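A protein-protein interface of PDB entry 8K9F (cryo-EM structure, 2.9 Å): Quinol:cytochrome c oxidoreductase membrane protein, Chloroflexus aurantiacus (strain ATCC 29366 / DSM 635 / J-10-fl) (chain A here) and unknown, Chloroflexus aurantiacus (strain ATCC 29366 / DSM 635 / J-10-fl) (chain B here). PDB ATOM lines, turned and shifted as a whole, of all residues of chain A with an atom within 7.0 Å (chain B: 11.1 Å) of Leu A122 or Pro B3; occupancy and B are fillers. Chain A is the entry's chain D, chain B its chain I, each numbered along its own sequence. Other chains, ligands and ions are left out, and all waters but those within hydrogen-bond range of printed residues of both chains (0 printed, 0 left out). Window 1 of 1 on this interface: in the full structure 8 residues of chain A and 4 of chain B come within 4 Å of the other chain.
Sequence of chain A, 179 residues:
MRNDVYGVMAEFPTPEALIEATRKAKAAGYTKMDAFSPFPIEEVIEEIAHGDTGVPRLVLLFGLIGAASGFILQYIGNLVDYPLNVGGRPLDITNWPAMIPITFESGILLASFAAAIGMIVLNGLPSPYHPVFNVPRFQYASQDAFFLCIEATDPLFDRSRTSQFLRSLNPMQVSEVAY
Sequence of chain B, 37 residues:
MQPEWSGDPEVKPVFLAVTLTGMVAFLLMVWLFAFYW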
ATOM      1  N   THR A  53      -9.188 -21.048 -30.167  1.00  0.00           N
ATOM      2  CA  THR A  53     -10.233 -20.951 -29.156  1.00  0.00           C
ATOM      3  C   THR A  53     -11.235 -19.845 -29.460  1.00  0.00           C
ATOM      4  O   THR A  53     -12.446 -20.090 -29.483  1.00  0.00           O
ATOM      5  CB  THR A  53      -9.581 -20.715 -27.809  1.00  0.00           C
ATOM      6  OG1 THR A  53      -8.680 -19.612 -27.946  1.00  0.00           O
ATOM      7  CG2 THR A  53      -8.796 -21.943 -27.393  1.00  0.00           C
ATOM      8  N   GLY A  54     -10.757 -18.623 -29.690  1.00  0.00           N
ATOM      9  CA  GLY A  54     -11.607 -17.506 -30.034  1.00  0.00           C
ATOM     10  C   GLY A  54     -11.566 -16.332 -29.074  1.00  0.00           C
ATOM     11  O   GLY A  54     -11.818 -15.202 -29.502  1.00  0.00           O
ATOM     12  N   VAL A  55     -11.255 -16.554 -27.800  1.00  0.00           N
ATOM     13  CA  VAL A  55     -11.056 -15.431 -26.878  1.00  0.00           C
ATOM     14  C   VAL A  55      -9.818 -14.551 -27.114  1.00  0.00           C
ATOM     15  O   VAL A  55      -9.867 -13.392 -26.665  1.00  0.00           O
ATOM     16  CB  VAL A  55     -11.070 -15.904 -25.410  1.00  0.00           C
ATOM     17  CG1 VAL A  55     -12.168 -16.911 -25.164  1.00  0.00           C
ATOM     18  CG2 VAL A  55      -9.736 -16.406 -24.946  1.00  0.00           C
ATOM     19  N   PRO A  56      -8.693 -14.975 -27.748  1.00  0.00           N
ATOM     20  CA  PRO A  56      -7.583 -14.014 -27.855  1.00  0.00           C
ATOM     21  C   PRO A  56      -7.846 -12.870 -28.814  1.00  0.00           C
ATOM     22  O   PRO A  56      -7.372 -11.755 -28.570  1.00  0.00           O
ATOM     23  CB  PRO A  56      -6.408 -14.877 -28.316  1.00  0.00           C
ATOM     24  CG  PRO A  56      -6.764 -16.187 -27.979  1.00  0.00           C
ATOM     25  CD  PRO A  56      -8.189 -16.261 -28.279  1.00  0.00           C
ATOM     26  N   LEU A  58     -10.756 -11.536 -29.137  1.00  0.00           N
ATOM     27  CA  LEU A  58     -11.614 -10.686 -28.317  1.00  0.00           C
ATOM     28  C   LEU A  58     -10.810  -9.817 -27.365  1.00  0.00           C
ATOM     29  O   LEU A  58     -11.094  -8.620 -27.231  1.00  0.00           O
ATOM     30  CB  LEU A  58     -12.602 -11.530 -27.520  1.00  0.00           C
ATOM     31  CG  LEU A  58     -13.416 -12.524 -28.323  1.00  0.00           C
ATOM     32  CD1 LEU A  58     -14.282 -13.309 -27.378  1.00  0.00           C
ATOM     33  CD2 LEU A  58     -14.250 -11.786 -29.344  1.00  0.00           C
ATOM     34  N   ALA A 116     -12.882 -12.718 -19.651  1.00  0.00           N
ATOM     35  CA  ALA A 116     -13.888 -13.365 -18.810  1.00  0.00           C
ATOM     36  C   ALA A 116     -15.187 -13.609 -19.565  1.00  0.00           C
ATOM     37  O   ALA A 116     -15.633 -14.755 -19.707  1.00  0.00           O
ATOM     38  CB  ALA A 116     -14.168 -12.507 -17.583  1.00  0.00           C
ATOM     39  N   ILE A 117     -15.806 -12.532 -20.057  1.00  0.00           N
ATOM     40  CA  ILE A 117     -17.114 -12.627 -20.687  1.00  0.00           C
ATOM     41  C   ILE A 117     -17.025 -13.378 -22.011  1.00  0.00           C
ATOM     42  O   ILE A 117     -17.939 -14.128 -22.360  1.00  0.00           O
ATOM     43  CB  ILE A 117     -17.709 -11.205 -20.808  1.00  0.00           C
ATOM     44  CG1 ILE A 117     -18.141 -10.720 -19.417  1.00  0.00           C
ATOM     45  CG2 ILE A 117     -18.868 -11.123 -21.809  1.00  0.00           C
ATOM     46  CD1 ILE A 117     -19.044  -9.492 -19.398  1.00  0.00           C
ATOM     47  N   GLY A 118     -15.904 -13.279 -22.727  1.00  0.00           N
ATOM     48  CA  GLY A 118     -15.762 -14.006 -23.972  1.00  0.00           C
ATOM     49  C   GLY A 118     -15.565 -15.494 -23.779  1.00  0.00           C
ATOM     50  O   GLY A 118     -16.076 -16.292 -24.562  1.00  0.00           O
ATOM     51  N   MET A 119     -14.824 -15.896 -22.741  1.00  0.00           N
ATOM     52  CA  MET A 119     -14.733 -17.320 -22.440  1.00  0.00           C
ATOM     53  C   MET A 119     -16.069 -17.871 -21.946  1.00  0.00           C
ATOM     54  O   MET A 119     -16.499 -18.950 -22.372  1.00  0.00           O
ATOM     55  CB  MET A 119     -13.633 -17.570 -21.414  1.00  0.00           C
ATOM     56  CG  MET A 119     -13.599 -19.001 -21.007  1.00  0.00           C
ATOM     57  SD  MET A 119     -14.104 -19.128 -19.309  1.00  0.00           S
ATOM     58  CE  MET A 119     -13.784 -20.843 -19.066  1.00  0.00           C
ATOM     59  N   ILE A 120     -16.753 -17.128 -21.070  1.00  0.00           N
ATOM     60  CA  ILE A 120     -18.051 -17.554 -20.551  1.00  0.00           C
ATOM     61  C   ILE A 120     -19.115 -17.571 -21.659  1.00  0.00           C
ATOM     62  O   ILE A 120     -20.018 -18.414 -21.658  1.00  0.00           O
ATOM     63  CB  ILE A 120     -18.412 -16.641 -19.356  1.00  0.00           C
ATOM     64  CG1 ILE A 120     -17.530 -16.949 -18.142  1.00  0.00           C
ATOM     65  CG2 ILE A 120     -19.813 -16.843 -18.878  1.00  0.00           C
ATOM     66  CD1 ILE A 120     -17.331 -18.425 -17.861  1.00  0.00           C
ATOM     67  N   VAL A 121     -18.991 -16.707 -22.660  1.00  0.00           N
ATOM     68  CA  VAL A 121     -19.992 -16.663 -23.717  1.00  0.00           C
ATOM     69  C   VAL A 121     -19.673 -17.672 -24.820  1.00  0.00           C
ATOM     70  O   VAL A 121     -20.569 -18.368 -25.306  1.00  0.00           O
ATOM     71  CB  VAL A 121     -20.114 -15.213 -24.231  1.00  0.00           C
ATOM     72  CG1 VAL A 121     -20.543 -15.144 -25.679  1.00  0.00           C
ATOM     73  CG2 VAL A 121     -21.107 -14.450 -23.371  1.00  0.00           C
ATOM     74  N   LEU A 122     -18.396 -17.804 -25.202  1.00  0.00           N
ATOM     75  CA  LEU A 122     -18.023 -18.710 -26.287  1.00  0.00           C
ATOM     76  C   LEU A 122     -18.162 -20.174 -25.888  1.00  0.00           C
ATOM     77  O   LEU A 122     -18.371 -21.030 -26.753  1.00  0.00           O
ATOM     78  CB  LEU A 122     -16.591 -18.438 -26.746  1.00  0.00           C
ATOM     79  CG  LEU A 122     -16.312 -17.256 -27.677  1.00  0.00           C
ATOM     80  CD1 LEU A 122     -14.830 -16.973 -27.694  1.00  0.00           C
ATOM     81  CD2 LEU A 122     -16.811 -17.482 -29.078  1.00  0.00           C
ATOM     82  N   ASN A 123     -18.050 -20.483 -24.595  1.00  0.00           N
ATOM     83  CA  ASN A 123     -18.352 -21.830 -24.130  1.00  0.00           C
ATOM     84  C   ASN A 123     -19.841 -22.061 -23.952  1.00  0.00           C
ATOM     85  O   ASN A 123     -20.235 -23.180 -23.615  1.00  0.00           O
ATOM     86  CB  ASN A 123     -17.659 -22.121 -22.801  1.00  0.00           C
ATOM     87  CG  ASN A 123     -16.161 -22.185 -22.921  1.00  0.00           C
ATOM     88  OD1 ASN A 123     -15.631 -22.598 -23.947  1.00  0.00           O
ATOM     89  ND2 ASN A 123     -15.465 -21.776 -21.874  1.00  0.00           N
ATOM     90  N   GLY A 124     -20.664 -21.034 -24.142  1.00  0.00           N
ATOM     91  CA  GLY A 124     -22.056 -21.104 -23.752  1.00  0.00           C
ATOM     92  C   GLY A 124     -22.227 -21.309 -22.268  1.00  0.00           C
ATOM     93  O   GLY A 124     -23.177 -21.972 -21.845  1.00  0.00           O
ATOM     94  N   LEU A 125     -21.282 -20.803 -21.506  1.00  0.00           N
ATOM     95  CA  LEU A 125     -21.277 -21.130 -20.109  1.00  0.00           C
ATOM     96  C   LEU A 125     -22.419 -20.860 -19.209  1.00  0.00           C
ATOM     97  O   LEU A 125     -22.766 -21.753 -18.472  1.00  0.00           O
ATOM     98  CB  LEU A 125     -19.992 -20.747 -19.446  1.00  0.00           C
ATOM     99  CG  LEU A 125     -19.529 -21.969 -18.657  1.00  0.00           C
ATOM    100  CD1 LEU A 125     -18.738 -22.939 -19.511  1.00  0.00           C
ATOM    101  CD2 LEU A 125     -18.867 -21.653 -17.331  1.00  0.00           C
ATOM    102  N   PRO A 126     -23.010 -19.638 -19.230  1.00  0.00           N
ATOM    103  CA  PRO A 126     -24.116 -19.532 -18.239  1.00  0.00           C
ATOM    104  C   PRO A 126     -25.330 -20.370 -18.633  1.00  0.00           C
ATOM    105  O   PRO A 126     -26.357 -19.882 -19.090  1.00  0.00           O
ATOM    106  CB  PRO A 126     -24.434 -18.033 -18.235  1.00  0.00           C
ATOM    107  CG  PRO A 126     -23.431 -17.382 -19.087  1.00  0.00           C
ATOM    108  CD  PRO A 126     -22.932 -18.405 -20.030  1.00  0.00           C
ATOM    109  N   MET B   1     -11.478 -23.892 -33.225  1.00  0.00           N
ATOM    110  CA  MET B   1     -12.720 -24.148 -32.507  1.00  0.00           C
ATOM    111  C   MET B   1     -13.744 -23.057 -32.761  1.00  0.00           C
ATOM    112  O   MET B   1     -13.404 -21.884 -32.916  1.00  0.00           O
ATOM    113  CB  MET B   1     -12.472 -24.259 -31.002  1.00  0.00           C
ATOM    114  CG  MET B   1     -11.908 -25.591 -30.541  1.00  0.00           C
ATOM    115  SD  MET B   1     -11.309 -25.592 -28.835  1.00  0.00           S
ATOM    116  CE  MET B   1     -12.093 -24.139 -28.144  1.00  0.00           C
ATOM    117  N   GLN B   2     -15.003 -23.455 -32.789  1.00  0.00           N
ATOM    118  CA  GLN B   2     -16.134 -22.550 -32.881  1.00  0.00           C
ATOM    119  C   GLN B   2     -16.901 -22.615 -31.573  1.00  0.00           C
ATOM    120  O   GLN B   2     -16.781 -23.592 -30.825  1.00  0.00           O
ATOM    121  CB  GLN B   2     -17.046 -22.916 -34.064  1.00  0.00           C
ATOM    122  CG  GLN B   2     -17.126 -24.396 -34.383  1.00  0.00           C
ATOM    123  CD  GLN B   2     -17.830 -24.655 -35.701  1.00  0.00           C
ATOM    124  OE1 GLN B   2     -17.835 -23.806 -36.591  1.00  0.00           O
ATOM    125  NE2 GLN B   2     -18.430 -25.832 -35.832  1.00  0.00           N
ATOM    126  N   PRO B   3     -17.663 -21.568 -31.239  1.00  0.00           N
ATOM    127  CA  PRO B   3     -18.564 -21.659 -30.082  1.00  0.00           C
ATOM    128  C   PRO B   3     -19.682 -22.660 -30.307  1.00  0.00           C
ATOM    129  O   PRO B   3     -19.974 -23.024 -31.449  1.00  0.00           O
ATOM    130  CB  PRO B   3     -19.116 -20.236 -29.949  1.00  0.00           C
ATOM    131  CG  PRO B   3     -18.861 -19.603 -31.276  1.00  0.00           C
ATOM    132  CD  PRO B   3     -17.598 -20.194 -31.765  1.00  0.00           C
ATOM    133  N   GLU B   4     -20.316 -23.114 -29.232  1.00  0.00           N
ATOM    134  CA  GLU B   4     -21.392 -24.082 -29.373  1.00  0.00           C
ATOM    135  C   GLU B   4     -22.712 -23.451 -29.787  1.00  0.00           C
ATOM    136  O   GLU B   4     -23.661 -24.181 -30.092  1.00  0.00           O
ATOM    137  CB  GLU B   4     -21.591 -24.853 -28.072  1.00  0.00           C
ATOM    138  CG  GLU B   4     -22.324 -24.089 -27.003  1.00  0.00           C
ATOM    139  CD  GLU B   4     -22.009 -24.618 -25.631  1.00  0.00           C
ATOM    140  OE1 GLU B   4     -20.985 -25.321 -25.495  1.00  0.00           O
ATOM    141  OE2 GLU B   4     -22.781 -24.341 -24.685  1.00  0.00           O
ATOM    142  N   TRP B   5     -22.805 -22.124 -29.799  1.00  0.00           N
ATOM    143  CA  TRP B   5     -23.983 -21.443 -30.308  1.00  0.00           C
ATOM    144  C   TRP B   5     -23.770 -20.908 -31.717  1.00  0.00           C
ATOM    145  O   TRP B   5     -24.557 -20.080 -32.184  1.00  0.00           O
ATOM    146  CB  TRP B   5     -24.402 -20.324 -29.352  1.00  0.00           C
ATOM    147  CG  TRP B   5     -23.276 -19.551 -28.732  1.00  0.00           C
ATOM    148  CD1 TRP B   5     -22.908 -19.573 -27.424  1.00  0.00           C
ATOM    149  CD2 TRP B   5     -22.443 -18.567 -29.364  1.00  0.00           C
ATOM    150  NE1 TRP B   5     -21.867 -18.712 -27.211  1.00  0.00           N
ATOM    151  CE2 TRP B   5     -21.568 -18.075 -28.385  1.00  0.00           C
ATOM    152  CE3 TRP B   5     -22.341 -18.072 -30.664  1.00  0.00           C
ATOM    153  CZ2 TRP B   5     -20.600 -17.119 -28.665  1.00  0.00           C
ATOM    154  CZ3 TRP B   5     -21.391 -17.119 -30.939  1.00  0.00           C
ATOM    155  CH2 TRP B   5     -20.527 -16.652 -29.946  1.00  0.00           C
ATOM    156  N   SER B   6     -22.703 -21.353 -32.390  1.00  0.00           N
ATOM    157  CA  SER B   6     -22.408 -20.880 -33.739  1.00  0.00           C
ATOM    158  C   SER B   6     -23.441 -21.359 -34.748  1.00  0.00           C
ATOM    159  O   SER B   6     -23.827 -20.603 -35.647  1.00  0.00           O
ATOM    160  CB  SER B   6     -21.017 -21.344 -34.164  1.00  0.00           C
ATOM    161  OG  SER B   6     -20.848 -22.725 -33.903  1.00  0.00           O
ATOM    162  N   GLY B   7     -23.900 -22.600 -34.616  1.00  0.00           N
ATOM    163  CA  GLY B   7     -24.877 -23.145 -35.532  1.00  0.00           C
ATOM    164  C   GLY B   7     -26.268 -23.207 -34.940  1.00  0.00           C
ATOM    165  O   GLY B   7     -26.993 -24.186 -35.141  1.00  0.00           O
ATOM    166  N   ASP B   8     -26.645 -22.173 -34.199  1.00  0.00           N
ATOM    167  CA  ASP B   8     -27.963 -22.117 -33.598  1.00  0.00           C
ATOM    168  C   ASP B   8     -28.791 -21.018 -34.248  1.00  0.00           C
ATOM    169  O   ASP B   8     -28.245 -19.973 -34.614  1.00  0.00           O
ATOM    170  CB  ASP B   8     -27.874 -21.856 -32.091  1.00  0.00           C
ATOM    171  CG  ASP B   8     -27.340 -23.047 -31.322  1.00  0.00           C
ATOM    172  OD1 ASP B   8     -27.303 -24.160 -31.889  1.00  0.00           O
ATOM    173  OD2 ASP B   8     -26.958 -22.869 -30.145  1.00  0.00           O
ATOM    174  N   PRO B   9     -30.101 -21.227 -34.421  1.00  0.00           N
ATOM    175  CA  PRO B   9     -30.949 -20.159 -34.977  1.00  0.00           C
ATOM    176  C   PRO B   9     -31.097 -18.955 -34.063  1.00  0.00           C
ATOM    177  O   PRO B   9     -31.470 -17.878 -34.544  1.00  0.00           O
ATOM    178  CB  PRO B   9     -32.298 -20.860 -35.198  1.00  0.00           C
ATOM    179  CG  PRO B   9     -31.955 -22.326 -35.267  1.00  0.00           C
ATOM    180  CD  PRO B   9     -30.850 -22.485 -34.263  1.00  0.00           C
ATOM    181  N   VAL B  11     -28.628 -17.394 -32.714  1.00  0.00           N
ATOM    182  CA  VAL B  11     -27.436 -16.550 -32.753  1.00  0.00           C
ATOM    183  C   VAL B  11     -27.649 -15.287 -33.584  1.00  0.00           C
ATOM    184  O   VAL B  11     -26.953 -14.287 -33.367  1.00  0.00           O
ATOM    185  CB  VAL B  11     -26.209 -17.354 -33.245  1.00  0.00           C
ATOM    186  CG1 VAL B  11     -26.134 -17.434 -34.766  1.00  0.00           C
ATOM    187  CG2 VAL B  11     -24.934 -16.755 -32.694  1.00  0.00           C
ATOM    188  N   PHE B  15     -27.860 -11.753 -30.950  1.00  0.00           N
ATOM    189  CA  PHE B  15     -26.770 -10.809 -31.159  1.00  0.00           C
ATOM    190  C   PHE B  15     -27.227  -9.554 -31.888  1.00  0.00           C
ATOM    191  O   PHE B  15     -26.523  -8.542 -31.848  1.00  0.00           O
ATOM    192  CB  PHE B  15     -25.617 -11.476 -31.904  1.00  0.00           C
ATOM    193  CG  PHE B  15     -24.646 -12.171 -31.000  1.00  0.00           C
ATOM    194  CD1 PHE B  15     -23.835 -11.440 -30.144  1.00  0.00           C
ATOM    195  CD2 PHE B  15     -24.549 -13.552 -30.992  1.00  0.00           C
ATOM    196  CE1 PHE B  15     -22.943 -12.070 -29.304  1.00  0.00           C
ATOM    197  CE2 PHE B  15     -23.654 -14.190 -30.151  1.00  0.00           C
ATOM    198  CZ  PHE B  15     -22.852 -13.449 -29.308  1.00  0.00           C
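The indole nitrogen of Trp B5 lies close to the backbone carbonyl oxygen of Val A121. The side-chain carboxylate (OE1) of Glu B4 sits close to the backbone carbonyl oxygen (O) of Asn A123, at 2.9 Å.
O of Met A119 lies within hydrogen-bond range of ND2 of Asn A123, 3.1 Å away. The side-chain hydroxyl of Ser B6 lies within hydrogen-bond range of the backbone carbonyl oxygen of Pro B3 (2.6 Å).
Among the printed residues, merely in contact across the chains: Thr A53 with Met B1 (3.8 Å), Leu A122 with Pro B3 (3.4 Å), Leu A122 with Glu B4 (3.8 Å), Leu A122 with Trp B5 (3.8 Å) and Gly A124 with Glu B4 (3.4 Å).
Of the printed residues of chain B, Thr A53 touches Met B1 (3.8 Å). Gly A54 touches none of the printed residues of chain B. No residue of chain B comes within 4 Å of Gly A118. Of the printed residues of chain B, Val A121 touches Trp B5 (2.3 Å). Of chain B, only Pro B3, Glu B4 and Trp B5 come within 4 Å of Leu A122. Asn A123 touches one residue of chain B. Of chain B, only Glu B4 (3.4 Å) comes within 4 Å of Gly A124. Of the printed residues of chain A, Met B1 touches Thr A53 (3.8 Å). Of chain A, only Leu A122 comes within 4 Å of Pro B3. Of the printed residues of chain A, Glu B4 touches Leu A122 (3.8 Å), Asn A123 (2.9 Å) and Gly A124 (3.4 Å). Of the printed residues of chain A, Trp B5 touches Val A121 (2.3 Å) and Leu A122 (3.8 Å). The nearest residue of chain B that does not touch Leu A122 is Gln B2 (5.1 Å). The nearest residue of chain A that does not touch Pro B3 is Val A121 (5.2 Å).
Hydrophobic or aromatic side chains of chain A within 4 Å of the printed part of chain B: Val A121 and Leu A122. Of the 11 printed residues of chain B, 4 touch a printed residue of chain A. Hydrophobic or aromatic side chains of chain B that line the printed part of chain A: Met B1, Pro B3 and Trp B5. Among the printed residues, 7 pairs touch across the chains.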
